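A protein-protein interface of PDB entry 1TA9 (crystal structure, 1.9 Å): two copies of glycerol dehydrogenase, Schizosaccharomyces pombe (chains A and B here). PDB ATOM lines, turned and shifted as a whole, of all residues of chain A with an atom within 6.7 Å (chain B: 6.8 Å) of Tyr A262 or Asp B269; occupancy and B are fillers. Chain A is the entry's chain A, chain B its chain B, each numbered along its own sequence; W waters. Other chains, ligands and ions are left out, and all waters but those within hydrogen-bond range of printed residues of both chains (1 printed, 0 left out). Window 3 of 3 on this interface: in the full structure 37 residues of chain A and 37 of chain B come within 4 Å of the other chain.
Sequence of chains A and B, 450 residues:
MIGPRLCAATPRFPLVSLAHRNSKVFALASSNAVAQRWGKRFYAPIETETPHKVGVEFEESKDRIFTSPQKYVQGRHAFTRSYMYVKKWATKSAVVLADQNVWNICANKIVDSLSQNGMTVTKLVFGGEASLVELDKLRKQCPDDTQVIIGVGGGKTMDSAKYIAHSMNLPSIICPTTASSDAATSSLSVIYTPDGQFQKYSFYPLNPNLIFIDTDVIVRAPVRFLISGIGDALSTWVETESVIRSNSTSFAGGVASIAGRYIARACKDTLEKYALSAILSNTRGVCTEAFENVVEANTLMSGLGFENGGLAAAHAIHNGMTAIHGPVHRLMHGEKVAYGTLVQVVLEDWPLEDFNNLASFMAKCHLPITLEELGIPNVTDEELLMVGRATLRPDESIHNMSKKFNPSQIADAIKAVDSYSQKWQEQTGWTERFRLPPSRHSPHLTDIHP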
ATOM      1  N   GLU A 241      17.718  -7.355 -23.609  1.00  0.00           N
ATOM      2  CA  GLU A 241      18.642  -8.298 -24.226  1.00  0.00           C
ATOM      3  C   GLU A 241      19.465  -7.582 -25.295  1.00  0.00           C
ATOM      4  O   GLU A 241      20.674  -7.787 -25.396  1.00  0.00           O
ATOM      5  CB  GLU A 241      17.880  -9.470 -24.854  1.00  0.00           C
ATOM      6  CG  GLU A 241      17.450 -10.539 -23.862  1.00  0.00           C
ATOM      7  CD  GLU A 241      18.634 -11.215 -23.197  1.00  0.00           C
ATOM      8  OE1 GLU A 241      18.789 -11.071 -21.966  1.00  0.00           O
ATOM      9  OE2 GLU A 241      19.417 -11.884 -23.907  1.00  0.00           O
ATOM     10  N   ILE A 244      22.091  -5.366 -23.488  1.00  0.00           N
ATOM     11  CA  ILE A 244      23.133  -6.189 -22.893  1.00  0.00           C
ATOM     12  C   ILE A 244      24.035  -6.821 -23.955  1.00  0.00           C
ATOM     13  O   ILE A 244      25.260  -6.792 -23.829  1.00  0.00           O
ATOM     14  CB  ILE A 244      22.514  -7.304 -22.013  1.00  0.00           C
ATOM     15  CG1 ILE A 244      21.846  -6.677 -20.788  1.00  0.00           C
ATOM     16  CG2 ILE A 244      23.585  -8.300 -21.582  1.00  0.00           C
ATOM     17  CD1 ILE A 244      21.042  -7.654 -19.960  1.00  0.00           C
ATOM     18  N   SER A 257      24.040  -5.541 -14.967  1.00  0.00           N
ATOM     19  CA  SER A 257      24.235  -6.612 -14.004  1.00  0.00           C
ATOM     20  C   SER A 257      23.562  -7.878 -14.532  1.00  0.00           C
ATOM     21  O   SER A 257      22.723  -7.827 -15.438  1.00  0.00           O
ATOM     22  CB  SER A 257      23.619  -6.246 -12.650  1.00  0.00           C
ATOM     23  OG  SER A 257      22.209  -6.122 -12.739  1.00  0.00           O
ATOM     24  N   ILE A 258      23.952  -9.014 -13.972  1.00  0.00           N
ATOM     25  CA  ILE A 258      23.367 -10.295 -14.344  1.00  0.00           C
ATOM     26  C   ILE A 258      21.979 -10.352 -13.693  1.00  0.00           C
ATOM     27  O   ILE A 258      21.017 -10.854 -14.277  1.00  0.00           O
ATOM     28  CB  ILE A 258      24.248 -11.460 -13.825  1.00  0.00           C
ATOM     29  CG1 ILE A 258      25.557 -11.511 -14.629  1.00  0.00           C
ATOM     30  CG2 ILE A 258      23.493 -12.789 -13.922  1.00  0.00           C
ATOM     31  CD1 ILE A 258      26.602 -12.467 -14.060  1.00  0.00           C
ATOM     32  N   ALA A 259      21.880  -9.819 -12.479  1.00  0.00           N
ATOM     33  CA  ALA A 259      20.611  -9.814 -11.755  1.00  0.00           C
ATOM     34  C   ALA A 259      19.509  -9.171 -12.594  1.00  0.00           C
ATOM     35  O   ALA A 259      18.410  -9.713 -12.719  1.00  0.00           O
ATOM     36  CB  ALA A 259      20.765  -9.066 -10.438  1.00  0.00           C
ATOM     37  N   GLY A 260      19.810  -8.012 -13.173  1.00  0.00           N
ATOM     38  CA  GLY A 260      18.829  -7.322 -13.990  1.00  0.00           C
ATOM     39  C   GLY A 260      18.385  -8.160 -15.173  1.00  0.00           C
ATOM     40  O   GLY A 260      17.210  -8.152 -15.545  1.00  0.00           O
ATOM     41  N   ARG A 261      19.321  -8.896 -15.761  1.00  0.00           N
ATOM     42  CA  ARG A 261      19.002  -9.734 -16.912  1.00  0.00           C
ATOM     43  C   ARG A 261      18.031 -10.848 -16.531  1.00  0.00           C
ATOM     44  O   ARG A 261      17.132 -11.190 -17.297  1.00  0.00           O
ATOM     45  CB  ARG A 261      20.283 -10.336 -17.494  1.00  0.00           C
ATOM     46  CG  ARG A 261      20.105 -10.915 -18.877  1.00  0.00           C
ATOM     47  CD  ARG A 261      21.442 -11.332 -19.473  1.00  0.00           C
ATOM     48  NE  ARG A 261      21.308 -11.678 -20.884  1.00  0.00           N
ATOM     49  CZ  ARG A 261      22.324 -12.011 -21.674  1.00  0.00           C
ATOM     50  NH1 ARG A 261      23.562 -12.050 -21.188  1.00  0.00           N
ATOM     51  NH2 ARG A 261      22.104 -12.287 -22.958  1.00  0.00           N
ATOM     52  N   TYR A 262      18.213 -11.415 -15.347  1.00  0.00           N
ATOM     53  CA  TYR A 262      17.325 -12.476 -14.885  1.00  0.00           C
ATOM     54  C   TYR A 262      15.940 -11.961 -14.514  1.00  0.00           C
ATOM     55  O   TYR A 262      14.957 -12.700 -14.599  1.00  0.00           O
ATOM     56  CB  TYR A 262      17.943 -13.204 -13.693  1.00  0.00           C
ATOM     57  CG  TYR A 262      18.781 -14.382 -14.120  1.00  0.00           C
ATOM     58  CD1 TYR A 262      18.285 -15.683 -14.032  1.00  0.00           C
ATOM     59  CD2 TYR A 262      20.058 -14.194 -14.653  1.00  0.00           C
ATOM     60  CE1 TYR A 262      19.045 -16.776 -14.467  1.00  0.00           C
ATOM     61  CE2 TYR A 262      20.819 -15.271 -15.090  1.00  0.00           C
ATOM     62  CZ  TYR A 262      20.310 -16.560 -14.995  1.00  0.00           C
ATOM     63  OH  TYR A 262      21.074 -17.627 -15.429  1.00  0.00           O
ATOM     64  N   ILE A 263      15.854 -10.701 -14.097  1.00  0.00           N
ATOM     65  CA  ILE A 263      14.554 -10.136 -13.747  1.00  0.00           C
ATOM     66  C   ILE A 263      13.785  -9.886 -15.047  1.00  0.00           C
ATOM     67  O   ILE A 263      12.558 -10.036 -15.099  1.00  0.00           O
ATOM     68  CB  ILE A 263      14.709  -8.835 -12.928  1.00  0.00           C
ATOM     69  CG1 ILE A 263      15.407  -9.155 -11.599  1.00  0.00           C
ATOM     70  CG2 ILE A 263      13.333  -8.222 -12.647  1.00  0.00           C
ATOM     71  CD1 ILE A 263      15.722  -7.941 -10.736  1.00  0.00           C
ATOM     72  N   ALA A 264      14.508  -9.519 -16.100  1.00  0.00           N
ATOM     73  CA  ALA A 264      13.877  -9.306 -17.397  1.00  0.00           C
ATOM     74  C   ALA A 264      13.371 -10.674 -17.863  1.00  0.00           C
ATOM     75  O   ALA A 264      12.297 -10.781 -18.448  1.00  0.00           O
ATOM     76  CB  ALA A 264      14.883  -8.737 -18.395  1.00  0.00           C
ATOM     77  N   ARG A 265      14.147 -11.718 -17.585  1.00  0.00           N
ATOM     78  CA  ARG A 265      13.760 -13.078 -17.951  1.00  0.00           C
ATOM     79  C   ARG A 265      12.519 -13.493 -17.160  1.00  0.00           C
ATOM     80  O   ARG A 265      11.619 -14.153 -17.685  1.00  0.00           O
ATOM     81  CB  ARG A 265      14.890 -14.062 -17.643  1.00  0.00           C
ATOM     82  CG  ARG A 265      14.560 -15.497 -18.039  1.00  0.00           C
ATOM     83  CD  ARG A 265      14.570 -15.635 -19.548  1.00  0.00           C
ATOM     84  NE  ARG A 265      13.764 -16.758 -20.016  1.00  0.00           N
ATOM     85  CZ  ARG A 265      13.778 -17.209 -21.266  1.00  0.00           C
ATOM     86  NH1 ARG A 265      14.566 -16.634 -22.171  1.00  0.00           N
ATOM     87  NH2 ARG A 265      12.994 -18.222 -21.617  1.00  0.00           N
ATOM     88  N   ALA A 266      12.481 -13.119 -15.887  1.00  0.00           N
ATOM     89  CA  ALA A 266      11.345 -13.454 -15.039  1.00  0.00           C
ATOM     90  C   ALA A 266      10.081 -12.837 -15.629  1.00  0.00           C
ATOM     91  O   ALA A 266       9.011 -13.449 -15.626  1.00  0.00           O
ATOM     92  CB  ALA A 266      11.577 -12.935 -13.627  1.00  0.00           C
ATOM     93  N   CYS A 267      10.215 -11.615 -16.126  1.00  0.00           N
ATOM     94  CA  CYS A 267       9.098 -10.906 -16.731  1.00  0.00           C
ATOM     95  C   CYS A 267       8.610 -11.704 -17.939  1.00  0.00           C
ATOM     96  O   CYS A 267       7.425 -12.019 -18.055  1.00  0.00           O
ATOM     97  CB  CYS A 267       9.555  -9.510 -17.164  1.00  0.00           C
ATOM     98  SG  CYS A 267       8.264  -8.468 -17.858  1.00  0.00           S
ATOM     99  N   ALA B 259      10.180 -12.359  -8.694  1.00  0.00           N
ATOM    100  CA  ALA B 259      11.467 -11.719  -8.953  1.00  0.00           C
ATOM    101  C   ALA B 259      12.567 -12.247  -8.033  1.00  0.00           C
ATOM    102  O   ALA B 259      13.676 -12.540  -8.483  1.00  0.00           O
ATOM    103  CB  ALA B 259      11.334 -10.207  -8.798  1.00  0.00           C
ATOM    104  N   TYR B 262      13.799 -15.619  -9.089  1.00  0.00           N
ATOM    105  CA  TYR B 262      14.656 -15.604 -10.272  1.00  0.00           C
ATOM    106  C   TYR B 262      16.050 -15.078  -9.953  1.00  0.00           C
ATOM    107  O   TYR B 262      17.028 -15.464 -10.597  1.00  0.00           O
ATOM    108  CB  TYR B 262      14.018 -14.770 -11.387  1.00  0.00           C
ATOM    109  CG  TYR B 262      13.177 -15.598 -12.331  1.00  0.00           C
ATOM    110  CD1 TYR B 262      13.663 -15.966 -13.585  1.00  0.00           C
ATOM    111  CD2 TYR B 262      11.907 -16.044 -11.957  1.00  0.00           C
ATOM    112  CE1 TYR B 262      12.906 -16.756 -14.445  1.00  0.00           C
ATOM    113  CE2 TYR B 262      11.145 -16.834 -12.807  1.00  0.00           C
ATOM    114  CZ  TYR B 262      11.650 -17.186 -14.050  1.00  0.00           C
ATOM    115  OH  TYR B 262      10.899 -17.973 -14.891  1.00  0.00           O
ATOM    116  N   ILE B 263      16.151 -14.196  -8.964  1.00  0.00           N
ATOM    117  CA  ILE B 263      17.459 -13.672  -8.580  1.00  0.00           C
ATOM    118  C   ILE B 263      18.228 -14.795  -7.885  1.00  0.00           C
ATOM    119  O   ILE B 263      19.446 -14.893  -8.016  1.00  0.00           O
ATOM    120  CB  ILE B 263      17.327 -12.445  -7.649  1.00  0.00           C
ATOM    121  CG1 ILE B 263      16.603 -11.317  -8.396  1.00  0.00           C
ATOM    122  CG2 ILE B 263      18.709 -11.965  -7.209  1.00  0.00           C
ATOM    123  CD1 ILE B 263      16.290 -10.102  -7.543  1.00  0.00           C
ATOM    124  N   ALA B 264      17.510 -15.647  -7.153  1.00  0.00           N
ATOM    125  CA  ALA B 264      18.144 -16.779  -6.481  1.00  0.00           C
ATOM    126  C   ALA B 264      18.655 -17.726  -7.568  1.00  0.00           C
ATOM    127  O   ALA B 264      19.729 -18.315  -7.439  1.00  0.00           O
ATOM    128  CB  ALA B 264      17.144 -17.501  -5.583  1.00  0.00           C
ATOM    129  N   ARG B 265      17.881 -17.867  -8.639  1.00  0.00           N
ATOM    130  CA  ARG B 265      18.272 -18.729  -9.750  1.00  0.00           C
ATOM    131  C   ARG B 265      19.505 -18.136 -10.433  1.00  0.00           C
ATOM    132  O   ARG B 265      20.412 -18.863 -10.837  1.00  0.00           O
ATOM    133  CB  ARG B 265      17.131 -18.850 -10.766  1.00  0.00           C
ATOM    134  CG  ARG B 265      17.458 -19.758 -11.944  1.00  0.00           C
ATOM    135  CD  ARG B 265      17.416 -21.224 -11.549  1.00  0.00           C
ATOM    136  NE  ARG B 265      18.226 -22.056 -12.436  1.00  0.00           N
ATOM    137  CZ  ARG B 265      18.237 -23.386 -12.411  1.00  0.00           C
ATOM    138  NH1 ARG B 265      17.469 -24.043 -11.546  1.00  0.00           N
ATOM    139  NH2 ARG B 265      19.032 -24.059 -13.233  1.00  0.00           N
ATOM    140  N   ALA B 266      19.528 -16.811 -10.561  1.00  0.00           N
ATOM    141  CA  ALA B 266      20.653 -16.119 -11.175  1.00  0.00           C
ATOM    142  C   ALA B 266      21.916 -16.457 -10.395  1.00  0.00           C
ATOM    143  O   ALA B 266      22.984 -16.680 -10.972  1.00  0.00           O
ATOM    144  CB  ALA B 266      20.412 -14.607 -11.167  1.00  0.00           C
ATOM    145  N   CYS B 267      21.784 -16.500  -9.076  1.00  0.00           N
ATOM    146  CA  CYS B 267      22.905 -16.830  -8.204  1.00  0.00           C
ATOM    147  C   CYS B 267      23.409 -18.245  -8.526  1.00  0.00           C
ATOM    148  O   CYS B 267      24.587 -18.444  -8.827  1.00  0.00           O
ATOM    149  CB  CYS B 267      22.455 -16.758  -6.744  1.00  0.00           C
ATOM    150  SG  CYS B 267      23.767 -17.029  -5.541  1.00  0.00           S
ATOM    151  N   LYS B 268      22.507 -19.218  -8.461  1.00  0.00           N
ATOM    152  CA  LYS B 268      22.843 -20.615  -8.745  1.00  0.00           C
ATOM    153  C   LYS B 268      23.521 -20.774 -10.109  1.00  0.00           C
ATOM    154  O   LYS B 268      24.577 -21.399 -10.226  1.00  0.00           O
ATOM    155  CB  LYS B 268      21.571 -21.468  -8.710  1.00  0.00           C
ATOM    156  CG  LYS B 268      21.767 -22.939  -9.070  1.00  0.00           C
ATOM    157  CD  LYS B 268      20.422 -23.660  -9.102  1.00  0.00           C
ATOM    158  CE  LYS B 268      20.569 -25.164  -9.276  1.00  0.00           C
ATOM    159  NZ  LYS B 268      21.145 -25.524 -10.595  1.00  0.00           N
ATOM    160  N   ASP B 269      22.904 -20.204 -11.139  1.00  0.00           N
ATOM    161  CA  ASP B 269      23.430 -20.295 -12.498  1.00  0.00           C
ATOM    162  C   ASP B 269      24.805 -19.668 -12.670  1.00  0.00           C
ATOM    163  O   ASP B 269      25.666 -20.214 -13.365  1.00  0.00           O
ATOM    164  CB  ASP B 269      22.469 -19.633 -13.484  1.00  0.00           C
ATOM    165  CG  ASP B 269      21.202 -20.439 -13.702  1.00  0.00           C
ATOM    166  OD1 ASP B 269      20.340 -19.973 -14.477  1.00  0.00           O
ATOM    167  OD2 ASP B 269      21.066 -21.529 -13.104  1.00  0.00           O
ATOM    168  N   THR B 270      25.007 -18.511 -12.051  1.00  0.00           N
ATOM    169  CA  THR B 270      26.285 -17.809 -12.155  1.00  0.00           C
ATOM    170  C   THR B 270      27.412 -18.594 -11.490  1.00  0.00           C
ATOM    171  O   THR B 270      28.528 -18.675 -12.018  1.00  0.00           O
ATOM    172  CB  THR B 270      26.179 -16.407 -11.527  1.00  0.00           C
ATOM    173  OG1 THR B 270      25.166 -15.666 -12.219  1.00  0.00           O
ATOM    174  CG2 THR B 270      27.505 -15.658 -11.634  1.00  0.00           C
ATOM    175  N   LEU B 271      27.125 -19.181 -10.334  1.00  0.00           N
ATOM    176  CA  LEU B 271      28.142 -19.957  -9.639  1.00  0.00           C
ATOM    177  C   LEU B 271      28.526 -21.178 -10.473  1.00  0.00           C
ATOM    178  O   LEU B 271      29.704 -21.514 -10.596  1.00  0.00           O
ATOM    179  CB  LEU B 271      27.626 -20.405  -8.274  1.00  0.00           C
ATOM    180  CG  LEU B 271      27.346 -19.297  -7.256  1.00  0.00           C
ATOM    181  CD1 LEU B 271      26.777 -19.929  -5.995  1.00  0.00           C
ATOM    182  CD2 LEU B 271      28.636 -18.527  -6.940  1.00  0.00           C
ATOM    183  N   GLU B 272      27.527 -21.843 -11.042  1.00  0.00           N
ATOM    184  CA  GLU B 272      27.780 -23.019 -11.862  1.00  0.00           C
ATOM    185  C   GLU B 272      28.692 -22.699 -13.041  1.00  0.00           C
ATOM    186  O   GLU B 272      29.586 -23.471 -13.375  1.00  0.00           O
ATOM    187  CB  GLU B 272      26.460 -23.605 -12.372  1.00  0.00           C
ATOM    188  CG  GLU B 272      25.737 -24.451 -11.331  1.00  0.00           C
ATOM    189  CD  GLU B 272      24.447 -25.065 -11.854  1.00  0.00           C
ATOM    190  OE1 GLU B 272      24.421 -25.518 -13.022  1.00  0.00           O
ATOM    191  OE2 GLU B 272      23.462 -25.108 -11.089  1.00  0.00           O
ATOM    192  N   LYS B 273      28.475 -21.549 -13.662  1.00  0.00           N
ATOM    193  CA  LYS B 273      29.276 -21.159 -14.815  1.00  0.00           C
ATOM    194  C   LYS B 273      30.633 -20.559 -14.467  1.00  0.00           C
ATOM    195  O   LYS B 273      31.636 -20.872 -15.111  1.00  0.00           O
ATOM    196  CB  LYS B 273      28.528 -20.127 -15.664  1.00  0.00           C
ATOM    197  CG  LYS B 273      27.282 -20.627 -16.376  1.00  0.00           C
ATOM    198  CD  LYS B 273      26.618 -19.464 -17.114  1.00  0.00           C
ATOM    199  CE  LYS B 273      25.368 -19.894 -17.863  1.00  0.00           C
ATOM    200  NZ  LYS B 273      24.743 -18.724 -18.550  1.00  0.00           N
ATOM    201  N   TYR B 274      30.669 -19.725 -13.434  1.00  0.00           N
ATOM    202  CA  TYR B 274      31.891 -19.006 -13.096  1.00  0.00           C
ATOM    203  C   TYR B 274      32.599 -19.196 -11.755  1.00  0.00           C
ATOM    204  O   TYR B 274      33.655 -18.607 -11.545  1.00  0.00           O
ATOM    205  CB  TYR B 274      31.613 -17.513 -13.281  1.00  0.00           C
ATOM    206  CG  TYR B 274      31.067 -17.170 -14.648  1.00  0.00           C
ATOM    207  CD1 TYR B 274      31.896 -17.175 -15.766  1.00  0.00           C
ATOM    208  CD2 TYR B 274      29.714 -16.871 -14.829  1.00  0.00           C
ATOM    209  CE1 TYR B 274      31.400 -16.894 -17.034  1.00  0.00           C
ATOM    210  CE2 TYR B 274      29.203 -16.587 -16.101  1.00  0.00           C
ATOM    211  CZ  TYR B 274      30.056 -16.600 -17.197  1.00  0.00           C
ATOM    212  OH  TYR B 274      29.584 -16.309 -18.458  1.00  0.00           O
ATOM    213  N   MET B 301      23.222 -10.954  -5.910  1.00  0.00           N
ATOM    214  CA  MET B 301      22.294 -12.057  -6.156  1.00  0.00           C
ATOM    215  C   MET B 301      21.979 -12.873  -4.908  1.00  0.00           C
ATOM    216  O   MET B 301      20.812 -13.090  -4.568  1.00  0.00           O
ATOM    217  CB  MET B 301      22.841 -12.972  -7.250  1.00  0.00           C
ATOM    218  CG  MET B 301      22.999 -12.297  -8.604  1.00  0.00           C
ATOM    219  SD  MET B 301      23.666 -13.453  -9.803  1.00  0.00           S
ATOM    220  CE  MET B 301      25.154 -12.577 -10.389  1.00  0.00           C
HETATM  221  O   HOH W   1      23.599 -17.595 -16.310  1.00  0.00           O
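Water W1 bridges the side-chain hydroxyl of Tyr A262 (2.7 Å) and the side-chain amino group of Lys B273 (2.8 Å).
The side-chain carboxylate (OD1) of Asp B269 lies within hydrogen-bond range of the side-chain hydroxyl (OH) of Tyr A262, 2.6 Å away.
Printed residues of chain B that touch a printed residue of chain A: Tyr B262, Ile B263, Ala B266, Asp B269, Thr B270 and Met B301. Hydrophobic or aromatic side chains of chain B that line the printed part of chain A: Tyr B262, Ile B263, Ala B266 and Met B301. Along chain B the printed residues that touch a printed residue of chain A span positions 262 to 301.
OG1 of Thr B270 touches CG2 of Ile A258, 3.7 Å away. Ile A258 touches Met B301 (CB to CE, 3.7 Å). Tyr B262 touches Tyr A262. Ala B266 touches Tyr A262. CD1 of Ile A263 touches CD1 of Ile B263 (3.9 Å). Ala A266 touches Tyr B262.
OD2 of Asp B269 lies within salt-bridge range of NE of Arg B265, 3.0 Å away. The side-chain hydroxyl (OG1) of Thr B270 is in hydrogen-bond range of the backbone carbonyl oxygen (O) of Ala B266 (2.7 Å). The backbone NH of Cys B267 is in hydrogen-bond range of the side-chain sulfur of Met B301 (3.7 Å). The side-chain sulfur (SD) of Met B301 lies close to the side-chain hydroxyl (OG1) of Thr B270 (3.6 Å).
Tyr A262 touches its own counterpart, Tyr B262. Tyr A262 touches Ala B266, and with the chains exchanged Ala A266 touches Tyr B262. Ile A263 touches its own counterpart, Ile B263.
Tyr A262 touches just these residues of chain B: Tyr B262, Ala B266 and Asp B269. Asp B269 touches just one residue of chain A: Tyr A262. Of the printed residues of chain A, Met B301 touches Ile A258 (3.7 Å). Printed residues of chain A within 4 Å of Tyr B262: Tyr A262 and Ala A266. Of the printed residues of chain A, Ile B263 touches Ile A263 (3.9 Å). Glu A241 touches none of the printed residues of chain B. Lys B268 touches none of the printed residues of chain A. The nearest printed residue of chain A that does not touch Asp B269 is Ile A258 (6.9 Å).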
